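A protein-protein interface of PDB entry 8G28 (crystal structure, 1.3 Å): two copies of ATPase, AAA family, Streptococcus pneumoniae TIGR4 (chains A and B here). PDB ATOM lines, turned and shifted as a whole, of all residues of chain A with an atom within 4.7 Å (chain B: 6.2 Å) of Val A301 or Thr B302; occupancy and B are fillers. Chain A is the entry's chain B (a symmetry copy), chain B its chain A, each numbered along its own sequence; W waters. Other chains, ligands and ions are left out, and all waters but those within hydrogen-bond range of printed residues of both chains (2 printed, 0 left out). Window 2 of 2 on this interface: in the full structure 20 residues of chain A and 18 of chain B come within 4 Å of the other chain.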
ATOM      1  N   THR A 282     -19.834 -12.616   5.235  1.00  0.00           N
ATOM      2  CA  THR A 282     -18.360 -12.693   5.125  1.00  0.00           C
ATOM      3  C   THR A 282     -17.771 -11.287   5.287  1.00  0.00           C
ATOM      4  O   THR A 282     -16.822 -11.098   6.062  1.00  0.00           O
ATOM      5  CB  THR A 282     -17.948 -13.345   3.801  1.00  0.00           C
ATOM      6  OG1 THR A 282     -18.506 -14.657   3.730  1.00  0.00           O
ATOM      7  CG2 THR A 282     -16.445 -13.432   3.663  1.00  0.00           C
ATOM      8  N   TYR A 286     -15.195  -9.557   8.510  1.00  0.00           N
ATOM      9  CA  TYR A 286     -13.888  -8.869   8.358  1.00  0.00           C
ATOM     10  C   TYR A 286     -13.988  -7.362   8.638  1.00  0.00           C
ATOM     11  O   TYR A 286     -12.985  -6.772   9.053  1.00  0.00           O
ATOM     12  CB  TYR A 286     -13.309  -9.135   6.965  1.00  0.00           C
ATOM     13  CG  TYR A 286     -12.796 -10.543   6.774  1.00  0.00           C
ATOM     14  CD1 TYR A 286     -13.617 -11.575   6.338  1.00  0.00           C
ATOM     15  CD2 TYR A 286     -11.468 -10.846   7.021  1.00  0.00           C
ATOM     16  CE1 TYR A 286     -13.132 -12.862   6.172  1.00  0.00           C
ATOM     17  CE2 TYR A 286     -10.966 -12.130   6.851  1.00  0.00           C
ATOM     18  CZ  TYR A 286     -11.801 -13.141   6.412  1.00  0.00           C
ATOM     19  OH  TYR A 286     -11.351 -14.425   6.271  1.00  0.00           O
ATOM     20  N   GLN A 297     -13.585 -14.979  11.740  1.00  0.00           N
ATOM     21  CA  GLN A 297     -13.517 -15.030  10.258  1.00  0.00           C
ATOM     22  C   GLN A 297     -13.343 -16.480   9.789  1.00  0.00           C
ATOM     23  O   GLN A 297     -13.982 -16.859   8.798  1.00  0.00           O
ATOM     24  CB  GLN A 297     -12.396 -14.147   9.715  1.00  0.00           C
ATOM     25  CG  GLN A 297     -12.658 -12.653   9.902  1.00  0.00           C
ATOM     26  CD  GLN A 297     -11.835 -12.014  10.994  1.00  0.00           C
ATOM     27  OE1 GLN A 297     -10.615 -12.134  11.023  1.00  0.00           O
ATOM     28  NE2 GLN A 297     -12.494 -11.315  11.898  1.00  0.00           N
ATOM     29  N   ILE A 298     -12.505 -17.268  10.463  1.00  0.00           N
ATOM     30  CA  ILE A 298     -12.338 -18.697  10.076  1.00  0.00           C
ATOM     31  C   ILE A 298     -13.689 -19.406  10.229  1.00  0.00           C
ATOM     32  O   ILE A 298     -14.088 -20.179   9.337  1.00  0.00           O
ATOM     33  CB  ILE A 298     -11.261 -19.373  10.941  1.00  0.00           C
ATOM     34  CG1 ILE A 298      -9.944 -18.597  10.941  1.00  0.00           C
ATOM     35  CG2 ILE A 298     -11.083 -20.818  10.520  1.00  0.00           C
ATOM     36  CD1 ILE A 298      -9.407 -18.309   9.579  1.00  0.00           C
ATOM     37  N   HIS A 299     -14.369 -19.188  11.350  1.00  0.00           N
ATOM     38  CA  HIS A 299     -15.674 -19.849  11.562  1.00  0.00           C
ATOM     39  C   HIS A 299     -16.645 -19.464  10.446  1.00  0.00           C
ATOM     40  O   HIS A 299     -17.399 -20.323   9.959  1.00  0.00           O
ATOM     41  CB  HIS A 299     -16.293 -19.433  12.899  1.00  0.00           C
ATOM     42  CG  HIS A 299     -15.478 -19.703  14.109  1.00  0.00           C
ATOM     43  ND1 HIS A 299     -15.675 -19.004  15.286  1.00  0.00           N
ATOM     44  CD2 HIS A 299     -14.401 -20.487  14.307  1.00  0.00           C
ATOM     45  CE1 HIS A 299     -14.788 -19.397  16.181  1.00  0.00           C
ATOM     46  NE2 HIS A 299     -14.010 -20.331  15.614  1.00  0.00           N
ATOM     47  N   THR A 300     -16.666 -18.181  10.101  1.00  0.00           N
ATOM     48  CA  THR A 300     -17.666 -17.653   9.148  1.00  0.00           C
ATOM     49  C   THR A 300     -17.421 -18.228   7.754  1.00  0.00           C
ATOM     50  O   THR A 300     -18.353 -18.756   7.128  1.00  0.00           O
ATOM     51  CB  THR A 300     -17.616 -16.123   9.128  1.00  0.00           C
ATOM     52  OG1 THR A 300     -18.027 -15.640  10.409  1.00  0.00           O
ATOM     53  CG2 THR A 300     -18.523 -15.531   8.072  1.00  0.00           C
ATOM     54  N   VAL A 301     -16.197 -18.100   7.262  1.00  0.00           N
ATOM     55  CA  VAL A 301     -15.912 -18.581   5.882  1.00  0.00           C
ATOM     56  C   VAL A 301     -16.126 -20.098   5.800  1.00  0.00           C
ATOM     57  O   VAL A 301     -16.727 -20.589   4.818  1.00  0.00           O
ATOM     58  CB  VAL A 301     -14.493 -18.179   5.457  1.00  0.00           C
ATOM     59  CG1 VAL A 301     -14.106 -18.848   4.150  1.00  0.00           C
ATOM     60  CG2 VAL A 301     -14.350 -16.664   5.364  1.00  0.00           C
ATOM     61  N   THR A 302     -15.678 -20.833   6.817  1.00  0.00           N
ATOM     62  CA  THR A 302     -15.803 -22.308   6.783  1.00  0.00           C
ATOM     63  C   THR A 302     -17.282 -22.701   6.741  1.00  0.00           C
ATOM     64  O   THR A 302     -17.688 -23.539   5.912  1.00  0.00           O
ATOM     65  CB  THR A 302     -15.107 -22.926   7.999  1.00  0.00           C
ATOM     66  OG1 THR A 302     -13.728 -22.559   7.982  1.00  0.00           O
ATOM     67  CG2 THR A 302     -15.243 -24.429   8.017  1.00  0.00           C
ATOM     68  N   ALA A 303     -18.088 -22.083   7.599  1.00  0.00           N
ATOM     69  CA  ALA A 303     -19.513 -22.470   7.706  1.00  0.00           C
ATOM     70  C   ALA A 303     -20.274 -22.060   6.448  1.00  0.00           C
ATOM     71  O   ALA A 303     -21.145 -22.819   6.005  1.00  0.00           O
ATOM     72  CB  ALA A 303     -20.136 -21.824   8.911  1.00  0.00           C
ATOM     73  N   LEU A 304     -19.981 -20.880   5.898  1.00  0.00           N
ATOM     74  CA  LEU A 304     -20.797 -20.407   4.750  1.00  0.00           C
ATOM     75  C   LEU A 304     -20.435 -21.193   3.487  1.00  0.00           C
ATOM     76  O   LEU A 304     -21.339 -21.499   2.699  1.00  0.00           O
ATOM     77  CB  LEU A 304     -20.634 -18.896   4.588  1.00  0.00           C
ATOM     78  CG  LEU A 304     -21.225 -18.068   5.728  1.00  0.00           C
ATOM     79  CD1 LEU A 304     -20.880 -16.602   5.542  1.00  0.00           C
ATOM     80  CD2 LEU A 304     -22.732 -18.256   5.827  1.00  0.00           C
ATOM     81  N   ASP A 305     -19.160 -21.536   3.315  1.00  0.00           N
ATOM     82  CA  ASP A 305     -18.787 -22.360   2.137  1.00  0.00           C
ATOM     83  C   ASP A 305     -19.480 -23.726   2.284  1.00  0.00           C
ATOM     84  O   ASP A 305     -20.026 -24.247   1.301  1.00  0.00           O
ATOM     85  CB  ASP A 305     -17.265 -22.464   2.008  1.00  0.00           C
ATOM     86  CG  ASP A 305     -16.568 -21.205   1.503  1.00  0.00           C
ATOM     87  OD1 ASP A 305     -17.271 -20.260   1.052  1.00  0.00           O
ATOM     88  OD2 ASP A 305     -15.317 -21.170   1.572  1.00  0.00           O
ATOM     89  N   GLN B 297      -0.757 -18.192   8.801  1.00  0.00           N
ATOM     90  CA  GLN B 297      -0.976 -18.802   7.464  1.00  0.00           C
ATOM     91  C   GLN B 297      -2.438 -19.233   7.305  1.00  0.00           C
ATOM     92  O   GLN B 297      -2.993 -19.051   6.214  1.00  0.00           O
ATOM     93  CB  GLN B 297      -0.044 -19.991   7.243  1.00  0.00           C
ATOM     94  CG  GLN B 297       1.416 -19.588   7.123  1.00  0.00           C
ATOM     95  CD  GLN B 297       2.246 -19.928   8.335  1.00  0.00           C
ATOM     96  OE1 GLN B 297       2.201 -21.046   8.842  1.00  0.00           O
ATOM     97  NE2 GLN B 297       3.043 -18.973   8.772  1.00  0.00           N
ATOM     98  N   ILE B 298      -3.045 -19.790   8.349  1.00  0.00           N
ATOM     99  CA  ILE B 298      -4.475 -20.200   8.250  1.00  0.00           C
ATOM    100  C   ILE B 298      -5.330 -18.961   7.973  1.00  0.00           C
ATOM    101  O   ILE B 298      -6.207 -19.001   7.083  1.00  0.00           O
ATOM    102  CB  ILE B 298      -4.932 -20.918   9.534  1.00  0.00           C
ATOM    103  CG1 ILE B 298      -4.010 -22.087   9.883  1.00  0.00           C
ATOM    104  CG2 ILE B 298      -6.384 -21.336   9.414  1.00  0.00           C
ATOM    105  CD1 ILE B 298      -3.766 -23.030   8.749  1.00  0.00           C
ATOM    106  N   HIS B 299      -5.089 -17.883   8.705  1.00  0.00           N
ATOM    107  CA  HIS B 299      -5.932 -16.681   8.501  1.00  0.00           C
ATOM    108  C   HIS B 299      -5.663 -16.052   7.129  1.00  0.00           C
ATOM    109  O   HIS B 299      -6.603 -15.512   6.521  1.00  0.00           O
ATOM    110  CB  HIS B 299      -5.711 -15.753   9.691  1.00  0.00           C
ATOM    111  CG  HIS B 299      -6.348 -16.271  10.934  1.00  0.00           C
ATOM    112  ND1 HIS B 299      -7.509 -15.725  11.427  1.00  0.00           N
ATOM    113  CD2 HIS B 299      -6.061 -17.328  11.731  1.00  0.00           C
ATOM    114  CE1 HIS B 299      -7.867 -16.366  12.523  1.00  0.00           C
ATOM    115  NE2 HIS B 299      -7.007 -17.360  12.723  1.00  0.00           N
ATOM    116  N   THR B 300      -4.420 -16.119   6.655  1.00  0.00           N
ATOM    117  CA  THR B 300      -4.075 -15.533   5.339  1.00  0.00           C
ATOM    118  C   THR B 300      -4.747 -16.319   4.209  1.00  0.00           C
ATOM    119  O   THR B 300      -5.405 -15.710   3.352  1.00  0.00           O
ATOM    120  CB  THR B 300      -2.555 -15.463   5.169  1.00  0.00           C
ATOM    121  OG1 THR B 300      -2.019 -14.582   6.156  1.00  0.00           O
ATOM    122  CG2 THR B 300      -2.155 -15.012   3.786  1.00  0.00           C
ATOM    123  N   VAL B 301      -4.549 -17.632   4.183  1.00  0.00           N
ATOM    124  CA  VAL B 301      -5.114 -18.422   3.058  1.00  0.00           C
ATOM    125  C   VAL B 301      -6.647 -18.336   3.089  1.00  0.00           C
ATOM    126  O   VAL B 301      -7.267 -18.175   2.029  1.00  0.00           O
ATOM    127  CB  VAL B 301      -4.600 -19.866   3.129  1.00  0.00           C
ATOM    128  CG1 VAL B 301      -5.315 -20.751   2.130  1.00  0.00           C
ATOM    129  CG2 VAL B 301      -3.095 -19.915   2.936  1.00  0.00           C
ATOM    130  N   THR B 302      -7.239 -18.406   4.277  1.00  0.00           N
ATOM    131  CA  THR B 302      -8.715 -18.358   4.373  1.00  0.00           C
ATOM    132  C   THR B 302      -9.215 -17.021   3.809  1.00  0.00           C
ATOM    133  O   THR B 302     -10.160 -17.003   2.999  1.00  0.00           O
ATOM    134  CB  THR B 302      -9.164 -18.539   5.830  1.00  0.00           C
ATOM    135  OG1 THR B 302      -8.721 -19.813   6.310  1.00  0.00           O
ATOM    136  CG2 THR B 302     -10.664 -18.417   5.974  1.00  0.00           C
ATOM    137  N   ALA B 303      -8.604 -15.922   4.242  1.00  0.00           N
ATOM    138  CA  ALA B 303      -9.062 -14.586   3.809  1.00  0.00           C
ATOM    139  C   ALA B 303      -8.850 -14.411   2.304  1.00  0.00           C
ATOM    140  O   ALA B 303      -9.720 -13.822   1.649  1.00  0.00           O
ATOM    141  CB  ALA B 303      -8.313 -13.515   4.555  1.00  0.00           C
ATOM    142  N   LEU B 304      -7.693 -14.830   1.794  1.00  0.00           N
ATOM    143  CA  LEU B 304      -7.374 -14.536   0.378  1.00  0.00           C
ATOM    144  C   LEU B 304      -8.225 -15.404  -0.556  1.00  0.00           C
ATOM    145  O   LEU B 304      -8.659 -14.889  -1.606  1.00  0.00           O
ATOM    146  CB  LEU B 304      -5.873 -14.709   0.147  1.00  0.00           C
ATOM    147  CG  LEU B 304      -4.997 -13.696   0.885  1.00  0.00           C
ATOM    148  CD1 LEU B 304      -3.526 -14.034   0.693  1.00  0.00           C
ATOM    149  CD2 LEU B 304      -5.298 -12.277   0.427  1.00  0.00           C
ATOM    150  N   ASP B 305      -8.483 -16.665  -0.199  1.00  0.00           N
ATOM    151  CA  ASP B 305      -9.386 -17.487  -1.046  1.00  0.00           C
ATOM    152  C   ASP B 305     -10.789 -16.856  -1.032  1.00  0.00           C
ATOM    153  O   ASP B 305     -11.433 -16.792  -2.091  1.00  0.00           O
ATOM    154  CB  ASP B 305      -9.358 -18.949  -0.597  1.00  0.00           C
ATOM    155  CG  ASP B 305      -8.084 -19.705  -0.948  1.00  0.00           C
ATOM    156  OD1 ASP B 305      -7.272 -19.190  -1.749  1.00  0.00           O
ATOM    157  OD2 ASP B 305      -7.931 -20.836  -0.443  1.00  0.00           O
ATOM    158  N   ALA B 306     -11.255 -16.393   0.129  1.00  0.00           N
ATOM    159  CA  ALA B 306     -12.584 -15.741   0.207  1.00  0.00           C
ATOM    160  C   ALA B 306     -12.559 -14.424  -0.582  1.00  0.00           C
ATOM    161  O   ALA B 306     -13.570 -14.089  -1.242  1.00  0.00           O
ATOM    162  CB  ALA B 306     -12.989 -15.514   1.647  1.00  0.00           C
ATOM    163  N   ALA B 307     -11.448 -13.692  -0.503  1.00  0.00           N
ATOM    164  CA  ALA B 307     -11.349 -12.388  -1.204  1.00  0.00           C
ATOM    165  C   ALA B 307     -11.466 -12.579  -2.716  1.00  0.00           C
ATOM    166  O   ALA B 307     -12.124 -11.763  -3.377  1.00  0.00           O
ATOM    167  CB  ALA B 307     -10.045 -11.716  -0.854  1.00  0.00           C
ATOM    168  N   LEU B 318     -10.963  -7.705   3.507  1.00  0.00           N
ATOM    169  CA  LEU B 318     -10.329  -9.003   3.854  1.00  0.00           C
ATOM    170  C   LEU B 318      -8.802  -8.852   3.790  1.00  0.00           C
ATOM    171  O   LEU B 318      -8.087  -9.280   4.700  1.00  0.00           O
ATOM    172  CB  LEU B 318     -10.836 -10.082   2.890  1.00  0.00           C
ATOM    173  CG  LEU B 318     -12.212 -10.665   3.215  1.00  0.00           C
ATOM    174  CD1 LEU B 318     -13.318  -9.626   3.182  1.00  0.00           C
ATOM    175  CD2 LEU B 318     -12.537 -11.795   2.262  1.00  0.00           C
HETATM  176  O   HOH W   1      -9.145 -15.100   7.662  1.00  0.00           O
HETATM  177  O   HOH W   2      -8.594 -13.621   9.907  1.00  0.00           O
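The backbone carbonyl oxygen of Ile B298 sits at hydrogen-bond distance from the side-chain hydroxyl of Thr B302 (2.8 Å).
The backbone carbonyl oxygen (O) of Ile A298 lies within hydrogen-bond range of the side-chain hydroxyl (OG1) of Thr A302 (2.8 Å).
Printed residues of chain B that touch a printed residue of chain A: His B299, Thr B302, Ala B303 and Leu B318.
Hydrophobic or aromatic side chains of chain B that line the printed part of chain A: His B299, Ala B303 and Leu B318.
Among the printed residues, 5 pairs touch across the chains.
Among the printed residues, no Asp or Glu carboxylate lies within 4 Å of a Lys or Arg side-chain nitrogen of the other chain.
Among the printed residues, merely in contact across the chains: Tyr A286 with Ala B303 (3.4 Å), Ile A298 with His B299 (3.4 Å), Tyr A286 with Leu B318 (3.5 Å), Ile A298 with Thr B302 (3.7 Å) and Val A301 with Thr B302 (3.9 Å).
Water W1 bridges OH of Tyr A286 (2.7 Å) and O of His B299 (2.8 Å).
Water W2 bridges OE1 of Gln A297 (2.7 Å) and ND1 of His B299 (2.8 Å).
Ile A298 touches His B299, but with the chains exchanged His A299 does not touch Ile B298 (8.5 Å).
Ile A298 touches Thr B302, but with the chains exchanged Thr A302 does not touch Ile B298 (7.6 Å).
Val A301 touches Thr B302, but with the chains exchanged Thr A302 does not touch Val B301 (9.6 Å).
Positions printed for both chains: 297, 298, 299, 300, 301, 302, 303, 304 and 305.
Of the printed residues of chain B, Tyr A286 touches Ala B303 (3.4 Å) and Leu B318 (3.5 Å).
Of the printed residues of chain B, Ile A298 touches His B299 (3.4 Å) and Thr B302 (3.7 Å).
Val A301 touches one residue of chain B.
Asp A305 touches none of the printed residues of chain B.
Ile B298 touches none of the printed residues of chain A.
Printed residues of chain A within 4 Å of His B299: Ile A298.
Thr B302 touches just these residues of chain A: Ile A298 and Val A301.
Printed residues of chain A within 4 Å of Ala B303: Tyr A286.
Of the printed residues of chain A, Leu B318 touches Tyr A286 (3.5 Å).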
